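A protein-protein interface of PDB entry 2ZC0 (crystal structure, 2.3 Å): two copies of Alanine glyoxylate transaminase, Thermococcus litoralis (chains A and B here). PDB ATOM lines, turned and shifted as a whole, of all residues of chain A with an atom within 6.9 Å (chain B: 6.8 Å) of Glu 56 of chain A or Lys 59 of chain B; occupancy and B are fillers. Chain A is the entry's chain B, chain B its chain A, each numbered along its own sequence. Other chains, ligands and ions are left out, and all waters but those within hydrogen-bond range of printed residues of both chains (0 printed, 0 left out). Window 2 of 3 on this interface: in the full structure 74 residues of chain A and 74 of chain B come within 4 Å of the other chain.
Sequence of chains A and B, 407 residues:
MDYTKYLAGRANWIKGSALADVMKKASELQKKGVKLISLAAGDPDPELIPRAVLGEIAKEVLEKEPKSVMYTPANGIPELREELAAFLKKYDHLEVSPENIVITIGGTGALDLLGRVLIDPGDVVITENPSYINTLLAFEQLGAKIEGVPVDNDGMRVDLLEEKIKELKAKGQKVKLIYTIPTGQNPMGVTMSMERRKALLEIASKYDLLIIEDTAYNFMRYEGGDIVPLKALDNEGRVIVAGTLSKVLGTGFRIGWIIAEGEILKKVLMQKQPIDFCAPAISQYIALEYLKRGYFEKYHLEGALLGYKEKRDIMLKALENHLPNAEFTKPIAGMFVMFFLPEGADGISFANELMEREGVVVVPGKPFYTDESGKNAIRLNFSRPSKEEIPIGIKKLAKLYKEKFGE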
ATOM      1  N   PRO A  50       0.389  26.007 -13.870  1.00  0.00           N
ATOM      2  CA  PRO A  50       0.397  24.579 -13.523  1.00  0.00           C
ATOM      3  C   PRO A  50       1.768  24.082 -13.082  1.00  0.00           C
ATOM      4  O   PRO A  50       2.367  23.218 -13.725  1.00  0.00           O
ATOM      5  CB  PRO A  50      -0.095  23.916 -14.809  1.00  0.00           C
ATOM      6  CG  PRO A  50       0.445  24.810 -15.875  1.00  0.00           C
ATOM      7  CD  PRO A  50       0.203  26.199 -15.323  1.00  0.00           C
ATOM      8  N   ARG A  51       2.258  24.626 -11.976  1.00  0.00           N
ATOM      9  CA  ARG A  51       3.573  24.255 -11.470  1.00  0.00           C
ATOM     10  C   ARG A  51       3.832  22.749 -11.461  1.00  0.00           C
ATOM     11  O   ARG A  51       4.866  22.292 -11.951  1.00  0.00           O
ATOM     12  CB  ARG A  51       3.774  24.825 -10.059  1.00  0.00           C
ATOM     13  CG  ARG A  51       3.734  26.341  -9.998  1.00  0.00           C
ATOM     14  CD  ARG A  51       4.789  26.867  -9.036  1.00  0.00           C
ATOM     15  NE  ARG A  51       4.679  26.299  -7.692  1.00  0.00           N
ATOM     16  CZ  ARG A  51       3.737  26.626  -6.814  1.00  0.00           C
ATOM     17  NH1 ARG A  51       3.720  26.061  -5.615  1.00  0.00           N
ATOM     18  NH2 ARG A  51       2.815  27.525  -7.130  1.00  0.00           N
ATOM     19  N   ALA A  52       2.890  21.990 -10.900  1.00  0.00           N
ATOM     20  CA  ALA A  52       2.990  20.531 -10.812  1.00  0.00           C
ATOM     21  C   ALA A  52       3.237  19.923 -12.186  1.00  0.00           C
ATOM     22  O   ALA A  52       4.186  19.172 -12.382  1.00  0.00           O
ATOM     23  CB  ALA A  52       1.707  19.959 -10.202  1.00  0.00           C
ATOM     24  N   VAL A  53       2.377  20.256 -13.140  1.00  0.00           N
ATOM     25  CA  VAL A  53       2.535  19.760 -14.496  1.00  0.00           C
ATOM     26  C   VAL A  53       3.924  20.108 -15.023  1.00  0.00           C
ATOM     27  O   VAL A  53       4.670  19.230 -15.466  1.00  0.00           O
ATOM     28  CB  VAL A  53       1.512  20.393 -15.441  1.00  0.00           C
ATOM     29  CG1 VAL A  53       1.731  19.875 -16.856  1.00  0.00           C
ATOM     30  CG2 VAL A  53       0.111  20.108 -14.956  1.00  0.00           C
ATOM     31  N   LEU A  54       4.271  21.392 -14.971  1.00  0.00           N
ATOM     32  CA  LEU A  54       5.572  21.830 -15.465  1.00  0.00           C
ATOM     33  C   LEU A  54       6.659  21.054 -14.746  1.00  0.00           C
ATOM     34  O   LEU A  54       7.715  20.769 -15.311  1.00  0.00           O
ATOM     35  CB  LEU A  54       5.766  23.341 -15.251  1.00  0.00           C
ATOM     36  CG  LEU A  54       4.832  24.305 -15.996  1.00  0.00           C
ATOM     37  CD1 LEU A  54       5.212  25.745 -15.668  1.00  0.00           C
ATOM     38  CD2 LEU A  54       4.920  24.067 -17.498  1.00  0.00           C
ATOM     39  N   GLY A  55       6.394  20.711 -13.490  1.00  0.00           N
ATOM     40  CA  GLY A  55       7.357  19.950 -12.712  1.00  0.00           C
ATOM     41  C   GLY A  55       7.511  18.566 -13.306  1.00  0.00           C
ATOM     42  O   GLY A  55       8.607  18.011 -13.348  1.00  0.00           O
ATOM     43  N   GLU A  56       6.396  18.011 -13.774  1.00  0.00           N
ATOM     44  CA  GLU A  56       6.391  16.685 -14.376  1.00  0.00           C
ATOM     45  C   GLU A  56       7.086  16.663 -15.734  1.00  0.00           C
ATOM     46  O   GLU A  56       7.882  15.765 -16.012  1.00  0.00           O
ATOM     47  CB  GLU A  56       4.952  16.172 -14.513  1.00  0.00           C
ATOM     48  CG  GLU A  56       4.338  15.713 -13.186  1.00  0.00           C
ATOM     49  CD  GLU A  56       4.797  14.323 -12.781  1.00  0.00           C
ATOM     50  OE1 GLU A  56       4.791  14.021 -11.565  1.00  0.00           O
ATOM     51  OE2 GLU A  56       5.153  13.527 -13.680  1.00  0.00           O
ATOM     52  N   ILE A  57       6.798  17.643 -16.584  1.00  0.00           N
ATOM     53  CA  ILE A  57       7.436  17.658 -17.890  1.00  0.00           C
ATOM     54  C   ILE A  57       8.938  17.955 -17.721  1.00  0.00           C
ATOM     55  O   ILE A  57       9.777  17.419 -18.453  1.00  0.00           O
ATOM     56  CB  ILE A  57       6.735  18.671 -18.869  1.00  0.00           C
ATOM     57  CG1 ILE A  57       7.642  19.848 -19.169  1.00  0.00           C
ATOM     58  CG2 ILE A  57       5.412  19.142 -18.305  1.00  0.00           C
ATOM     59  CD1 ILE A  57       8.466  19.611 -20.379  1.00  0.00           C
ATOM     60  N   ALA A  58       9.285  18.783 -16.738  1.00  0.00           N
ATOM     61  CA  ALA A  58      10.693  19.092 -16.486  1.00  0.00           C
ATOM     62  C   ALA A  58      11.432  17.789 -16.159  1.00  0.00           C
ATOM     63  O   ALA A  58      12.529  17.537 -16.665  1.00  0.00           O
ATOM     64  CB  ALA A  58      10.821  20.066 -15.325  1.00  0.00           C
ATOM     65  N   LYS A  59      10.826  16.970 -15.304  1.00  0.00           N
ATOM     66  CA  LYS A  59      11.408  15.686 -14.926  1.00  0.00           C
ATOM     67  C   LYS A  59      11.594  14.845 -16.188  1.00  0.00           C
ATOM     68  O   LYS A  59      12.695  14.383 -16.497  1.00  0.00           O
ATOM     69  CB  LYS A  59      10.473  14.950 -13.954  1.00  0.00           C
ATOM     70  CG  LYS A  59      10.912  13.543 -13.568  1.00  0.00           C
ATOM     71  CD  LYS A  59       9.782  12.763 -12.874  1.00  0.00           C
ATOM     72  CE  LYS A  59       8.892  11.970 -13.865  1.00  0.00           C
ATOM     73  NZ  LYS A  59       8.163  12.795 -14.883  1.00  0.00           N
ATOM     74  N   GLU A  60      10.502  14.671 -16.919  1.00  0.00           N
ATOM     75  CA  GLU A  60      10.497  13.886 -18.138  1.00  0.00           C
ATOM     76  C   GLU A  60      11.589  14.271 -19.120  1.00  0.00           C
ATOM     77  O   GLU A  60      12.426  13.438 -19.510  1.00  0.00           O
ATOM     78  CB  GLU A  60       9.145  14.033 -18.819  1.00  0.00           C
ATOM     79  CG  GLU A  60       9.017  13.255 -20.098  1.00  0.00           C
ATOM     80  CD  GLU A  60       7.665  13.466 -20.742  1.00  0.00           C
ATOM     81  OE1 GLU A  60       6.652  13.371 -20.012  1.00  0.00           O
ATOM     82  OE2 GLU A  60       7.613  13.725 -21.968  1.00  0.00           O
ATOM     83  N   VAL A  61      11.553  15.535 -19.534  1.00  0.00           N
ATOM     84  CA  VAL A  61      12.509  16.080 -20.482  1.00  0.00           C
ATOM     85  C   VAL A  61      13.933  15.806 -20.026  1.00  0.00           C
ATOM     86  O   VAL A  61      14.763  15.353 -20.809  1.00  0.00           O
ATOM     87  CB  VAL A  61      12.281  17.612 -20.663  1.00  0.00           C
ATOM     88  CG1 VAL A  61      13.459  18.244 -21.360  1.00  0.00           C
ATOM     89  CG2 VAL A  61      11.010  17.849 -21.477  1.00  0.00           C
ATOM     90  N   LEU A  62      14.220  16.068 -18.757  1.00  0.00           N
ATOM     91  CA  LEU A  62      15.565  15.833 -18.257  1.00  0.00           C
ATOM     92  C   LEU A  62      16.030  14.387 -18.340  1.00  0.00           C
ATOM     93  O   LEU A  62      17.196  14.134 -18.633  1.00  0.00           O
ATOM     94  CB  LEU A  62      15.698  16.335 -16.821  1.00  0.00           C
ATOM     95  CG  LEU A  62      15.897  17.845 -16.711  1.00  0.00           C
ATOM     96  CD1 LEU A  62      15.911  18.239 -15.256  1.00  0.00           C
ATOM     97  CD2 LEU A  62      17.207  18.249 -17.404  1.00  0.00           C
ATOM     98  N   ARG A 293       1.588  19.622 -25.950  1.00  0.00           N
ATOM     99  CA  ARG A 293       0.552  18.914 -25.199  1.00  0.00           C
ATOM    100  C   ARG A 293      -0.747  19.696 -25.000  1.00  0.00           C
ATOM    101  O   ARG A 293      -1.608  19.269 -24.234  1.00  0.00           O
ATOM    102  CB  ARG A 293       1.082  18.487 -23.829  1.00  0.00           C
ATOM    103  CG  ARG A 293       2.099  17.348 -23.854  1.00  0.00           C
ATOM    104  CD  ARG A 293       2.506  16.953 -22.432  1.00  0.00           C
ATOM    105  NE  ARG A 293       3.661  16.049 -22.437  1.00  0.00           N
ATOM    106  CZ  ARG A 293       4.325  15.658 -21.352  1.00  0.00           C
ATOM    107  NH1 ARG A 293       3.964  16.079 -20.148  1.00  0.00           N
ATOM    108  NH2 ARG A 293       5.357  14.862 -21.481  1.00  0.00           N
ATOM    109  N   LEU B  54      18.531  15.246 -11.562  1.00  0.00           N
ATOM    110  CA  LEU B  54      18.169  16.647 -11.806  1.00  0.00           C
ATOM    111  C   LEU B  54      16.691  16.749 -12.148  1.00  0.00           C
ATOM    112  O   LEU B  54      16.037  17.739 -11.830  1.00  0.00           O
ATOM    113  CB  LEU B  54      18.988  17.224 -12.955  1.00  0.00           C
ATOM    114  CG  LEU B  54      20.497  17.347 -12.766  1.00  0.00           C
ATOM    115  CD1 LEU B  54      21.099  17.968 -14.013  1.00  0.00           C
ATOM    116  CD2 LEU B  54      20.806  18.192 -11.524  1.00  0.00           C
ATOM    117  N   GLY B  55      16.185  15.714 -12.810  1.00  0.00           N
ATOM    118  CA  GLY B  55      14.790  15.683 -13.178  1.00  0.00           C
ATOM    119  C   GLY B  55      13.886  15.737 -11.959  1.00  0.00           C
ATOM    120  O   GLY B  55      13.018  16.602 -11.890  1.00  0.00           O
ATOM    121  N   GLU B  56      14.073  14.838 -10.991  1.00  0.00           N
ATOM    122  CA  GLU B  56      13.215  14.853  -9.807  1.00  0.00           C
ATOM    123  C   GLU B  56      13.395  16.123  -8.979  1.00  0.00           C
ATOM    124  O   GLU B  56      12.428  16.609  -8.395  1.00  0.00           O
ATOM    125  CB  GLU B  56      13.429  13.594  -8.916  1.00  0.00           C
ATOM    126  CG  GLU B  56      12.283  12.531  -9.011  1.00  0.00           C
ATOM    127  CD  GLU B  56      11.243  12.604  -7.867  1.00  0.00           C
ATOM    128  OE1 GLU B  56      10.101  12.080  -8.047  1.00  0.00           O
ATOM    129  OE2 GLU B  56      11.570  13.167  -6.788  1.00  0.00           O
ATOM    130  N   ILE B  57      14.609  16.671  -8.919  1.00  0.00           N
ATOM    131  CA  ILE B  57      14.788  17.901  -8.147  1.00  0.00           C
ATOM    132  C   ILE B  57      14.055  19.045  -8.867  1.00  0.00           C
ATOM    133  O   ILE B  57      13.461  19.917  -8.225  1.00  0.00           O
ATOM    134  CB  ILE B  57      16.291  18.251  -7.931  1.00  0.00           C
ATOM    135  CG1 ILE B  57      16.668  19.527  -8.668  1.00  0.00           C
ATOM    136  CG2 ILE B  57      17.157  17.118  -8.378  1.00  0.00           C
ATOM    137  CD1 ILE B  57      16.507  20.764  -7.834  1.00  0.00           C
ATOM    138  N   ALA B  58      14.072  19.011 -10.197  1.00  0.00           N
ATOM    139  CA  ALA B  58      13.385  20.022 -10.994  1.00  0.00           C
ATOM    140  C   ALA B  58      11.882  19.948 -10.706  1.00  0.00           C
ATOM    141  O   ALA B  58      11.226  20.972 -10.498  1.00  0.00           O
ATOM    142  CB  ALA B  58      13.654  19.792 -12.482  1.00  0.00           C
ATOM    143  N   LYS B  59      11.347  18.729 -10.682  1.00  0.00           N
ATOM    144  CA  LYS B  59       9.927  18.519 -10.402  1.00  0.00           C
ATOM    145  C   LYS B  59       9.584  18.992  -8.991  1.00  0.00           C
ATOM    146  O   LYS B  59       8.576  19.677  -8.782  1.00  0.00           O
ATOM    147  CB  LYS B  59       9.572  17.038 -10.525  1.00  0.00           C
ATOM    148  CG  LYS B  59       8.070  16.753 -10.529  1.00  0.00           C
ATOM    149  CD  LYS B  59       7.718  15.491  -9.753  1.00  0.00           C
ATOM    150  CE  LYS B  59       8.465  14.268 -10.258  1.00  0.00           C
ATOM    151  NZ  LYS B  59       8.150  13.072  -9.415  1.00  0.00           N
ATOM    152  N   GLU B  60      10.427  18.606  -8.033  1.00  0.00           N
ATOM    153  CA  GLU B  60      10.254  18.969  -6.628  1.00  0.00           C
ATOM    154  C   GLU B  60      10.227  20.487  -6.469  1.00  0.00           C
ATOM    155  O   GLU B  60       9.296  21.052  -5.882  1.00  0.00           O
ATOM    156  CB  GLU B  60      11.401  18.392  -5.784  1.00  0.00           C
ATOM    157  CG  GLU B  60      11.342  16.878  -5.533  1.00  0.00           C
ATOM    158  CD  GLU B  60      12.607  16.349  -4.844  1.00  0.00           C
ATOM    159  OE1 GLU B  60      12.611  15.173  -4.396  1.00  0.00           O
ATOM    160  OE2 GLU B  60      13.603  17.107  -4.754  1.00  0.00           O
ATOM    161  N   VAL B  61      11.261  21.135  -6.994  1.00  0.00           N
ATOM    162  CA  VAL B  61      11.377  22.583  -6.932  1.00  0.00           C
ATOM    163  C   VAL B  61      10.150  23.302  -7.500  1.00  0.00           C
ATOM    164  O   VAL B  61       9.621  24.222  -6.877  1.00  0.00           O
ATOM    165  CB  VAL B  61      12.635  23.069  -7.691  1.00  0.00           C
ATOM    166  CG1 VAL B  61      12.604  24.574  -7.837  1.00  0.00           C
ATOM    167  CG2 VAL B  61      13.894  22.645  -6.936  1.00  0.00           C
ATOM    168  N   LEU B  62       9.690  22.877  -8.674  1.00  0.00           N
ATOM    169  CA  LEU B  62       8.537  23.515  -9.311  1.00  0.00           C
ATOM    170  C   LEU B  62       7.218  23.384  -8.554  1.00  0.00           C
ATOM    171  O   LEU B  62       6.473  24.358  -8.421  1.00  0.00           O
ATOM    172  CB  LEU B  62       8.375  22.994 -10.741  1.00  0.00           C
ATOM    173  CG  LEU B  62       9.386  23.597 -11.723  1.00  0.00           C
ATOM    174  CD1 LEU B  62       9.568  22.707 -12.953  1.00  0.00           C
ATOM    175  CD2 LEU B  62       8.905  24.995 -12.106  1.00  0.00           C
ATOM    176  N   GLU B  63       6.927  22.193  -8.049  1.00  0.00           N
ATOM    177  CA  GLU B  63       5.677  21.992  -7.331  1.00  0.00           C
ATOM    178  C   GLU B  63       5.686  22.565  -5.911  1.00  0.00           C
ATOM    179  O   GLU B  63       4.653  23.025  -5.420  1.00  0.00           O
ATOM    180  CB  GLU B  63       5.325  20.497  -7.299  1.00  0.00           C
ATOM    181  CG  GLU B  63       6.323  19.619  -6.564  1.00  0.00           C
ATOM    182  CD  GLU B  63       6.002  18.129  -6.667  1.00  0.00           C
ATOM    183  OE1 GLU B  63       6.721  17.323  -6.031  1.00  0.00           O
ATOM    184  OE2 GLU B  63       5.040  17.762  -7.382  1.00  0.00           O
ATOM    185  N   LYS B  64       6.849  22.577  -5.263  1.00  0.00           N
ATOM    186  CA  LYS B  64       6.942  23.072  -3.886  1.00  0.00           C
ATOM    187  C   LYS B  64       7.327  24.545  -3.715  1.00  0.00           C
ATOM    188  O   LYS B  64       6.882  25.197  -2.769  1.00  0.00           O
ATOM    189  CB  LYS B  64       7.913  22.179  -3.096  1.00  0.00           C
ATOM    190  CG  LYS B  64       7.493  20.705  -3.078  1.00  0.00           C
ATOM    191  CD  LYS B  64       8.626  19.766  -2.663  1.00  0.00           C
ATOM    192  CE  LYS B  64       8.263  18.308  -2.968  1.00  0.00           C
ATOM    193  NZ  LYS B  64       9.320  17.336  -2.566  1.00  0.00           N
ATOM    194  N   ILE B 286      17.436  24.551  -9.236  1.00  0.00           N
ATOM    195  CA  ILE B 286      17.986  23.226  -9.495  1.00  0.00           C
ATOM    196  C   ILE B 286      19.425  23.187  -8.970  1.00  0.00           C
ATOM    197  O   ILE B 286      19.840  22.218  -8.328  1.00  0.00           O
ATOM    198  CB  ILE B 286      18.006  22.892 -11.005  1.00  0.00           C
ATOM    199  CG1 ILE B 286      16.593  22.601 -11.516  1.00  0.00           C
ATOM    200  CG2 ILE B 286      18.898  21.676 -11.260  1.00  0.00           C
ATOM    201  CD1 ILE B 286      16.563  22.169 -12.975  1.00  0.00           C
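Printed residues of chain A that touch a printed residue of chain B: Arg 51, Leu 54, Gly 55, Glu 56, Ala 58, Lys 59 and Leu 62.
Hydrophobic or aromatic side chains of chain A that line the printed part of chain B: Ala 58 and Leu 62.
Hydrophobic or aromatic side chains of chain B that line the printed part of chain A: Leu 54, Ala 58 and Leu 62.
Of the printed residues of chain B, Leu 54 of chain A touches Leu 62 (3.6 Å).
Of chain B, only Lys 59 (3.1 Å) and Leu 62 (3.5 Å) come within 4 Å of Gly 55 of chain A.
Of the printed residues of chain A, Gly 55 of chain B touches Lys 59 and Leu 62.
Of chain A, only Gly 55 (3.1 Å), Glu 56 (3.7 Å) and Lys 59 (3.3 Å) come within 4 Å of Lys 59 of chain B.
Of the printed residues of chain A, Leu 62 of chain B touches Arg 51, Leu 54, Gly 55 and Ala 58.
Of the printed residues of chain A, Glu 63 of chain B touches Arg 51.
The nearest residue of chain B that does not touch Glu 56 of chain A is Glu 63 of chain B (5.6 Å).
The backbone carbonyl oxygen of Leu 62 of chain B sits at hydrogen-bond distance from the guanidinium group of Arg 51 of chain A, at 2.7 Å.
O of Glu 63 of chain B is in hydrogen-bond range of NH1 of Arg 51 of chain A (3.2 Å).
Among the printed residues, pairs that only touch across the chains: Gly 55 of chain A with Lys 59 of chain B (3.1 Å), Lys 59 of chain A with Lys 59 of chain B (3.3 Å), Leu 62 of chain A with Leu 54 of chain B (3.5 Å), Leu 62 of chain A with Gly 55 of chain B (3.5 Å), Gly 55 of chain A with Leu 62 of chain B (3.5 Å), Lys 59 of chain A with Gly 55 of chain B (3.6 Å), Leu 54 of chain A with Leu 62 of chain B (3.6 Å), Glu 56 of chain A with Lys 59 of chain B (3.7 Å), Ala 58 of chain A with Leu 62 of chain B (3.8 Å) and Leu 62 of chain A with Ala 58 of chain B (3.9 Å).
OE1 of Glu 56 of chain B lies within salt-bridge range of NZ of Lys 59 of chain B (2.6 Å).
The side-chain carboxylate (OE2) of Glu 56 of chain A lies within salt-bridge range of the side-chain amino group (NZ) of Lys 59 of chain A (3.3 Å).
Leu 54 of chain A touches Leu 62 of chain B, and with the chains exchanged Leu 62 of chain A touches Leu 54 of chain B.
Gly 55 of chain A touches Leu 62 of chain B, and with the chains exchanged Leu 62 of chain A touches Gly 55 of chain B.
Glu 56 of chain A touches Lys 59 of chain B, but with the chains exchanged Lys 59 of chain A does not touch Glu 56 of chain B (4.3 Å).
Ala 58 of chain A touches Leu 62 of chain B, and with the chains exchanged Leu 62 of chain A touches Ala 58 of chain B.
9 positions are printed for both chains.
Of the 12 pairs that touch across the chains among the printed residues, 9 have their exchanged pair printed and touching as well.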
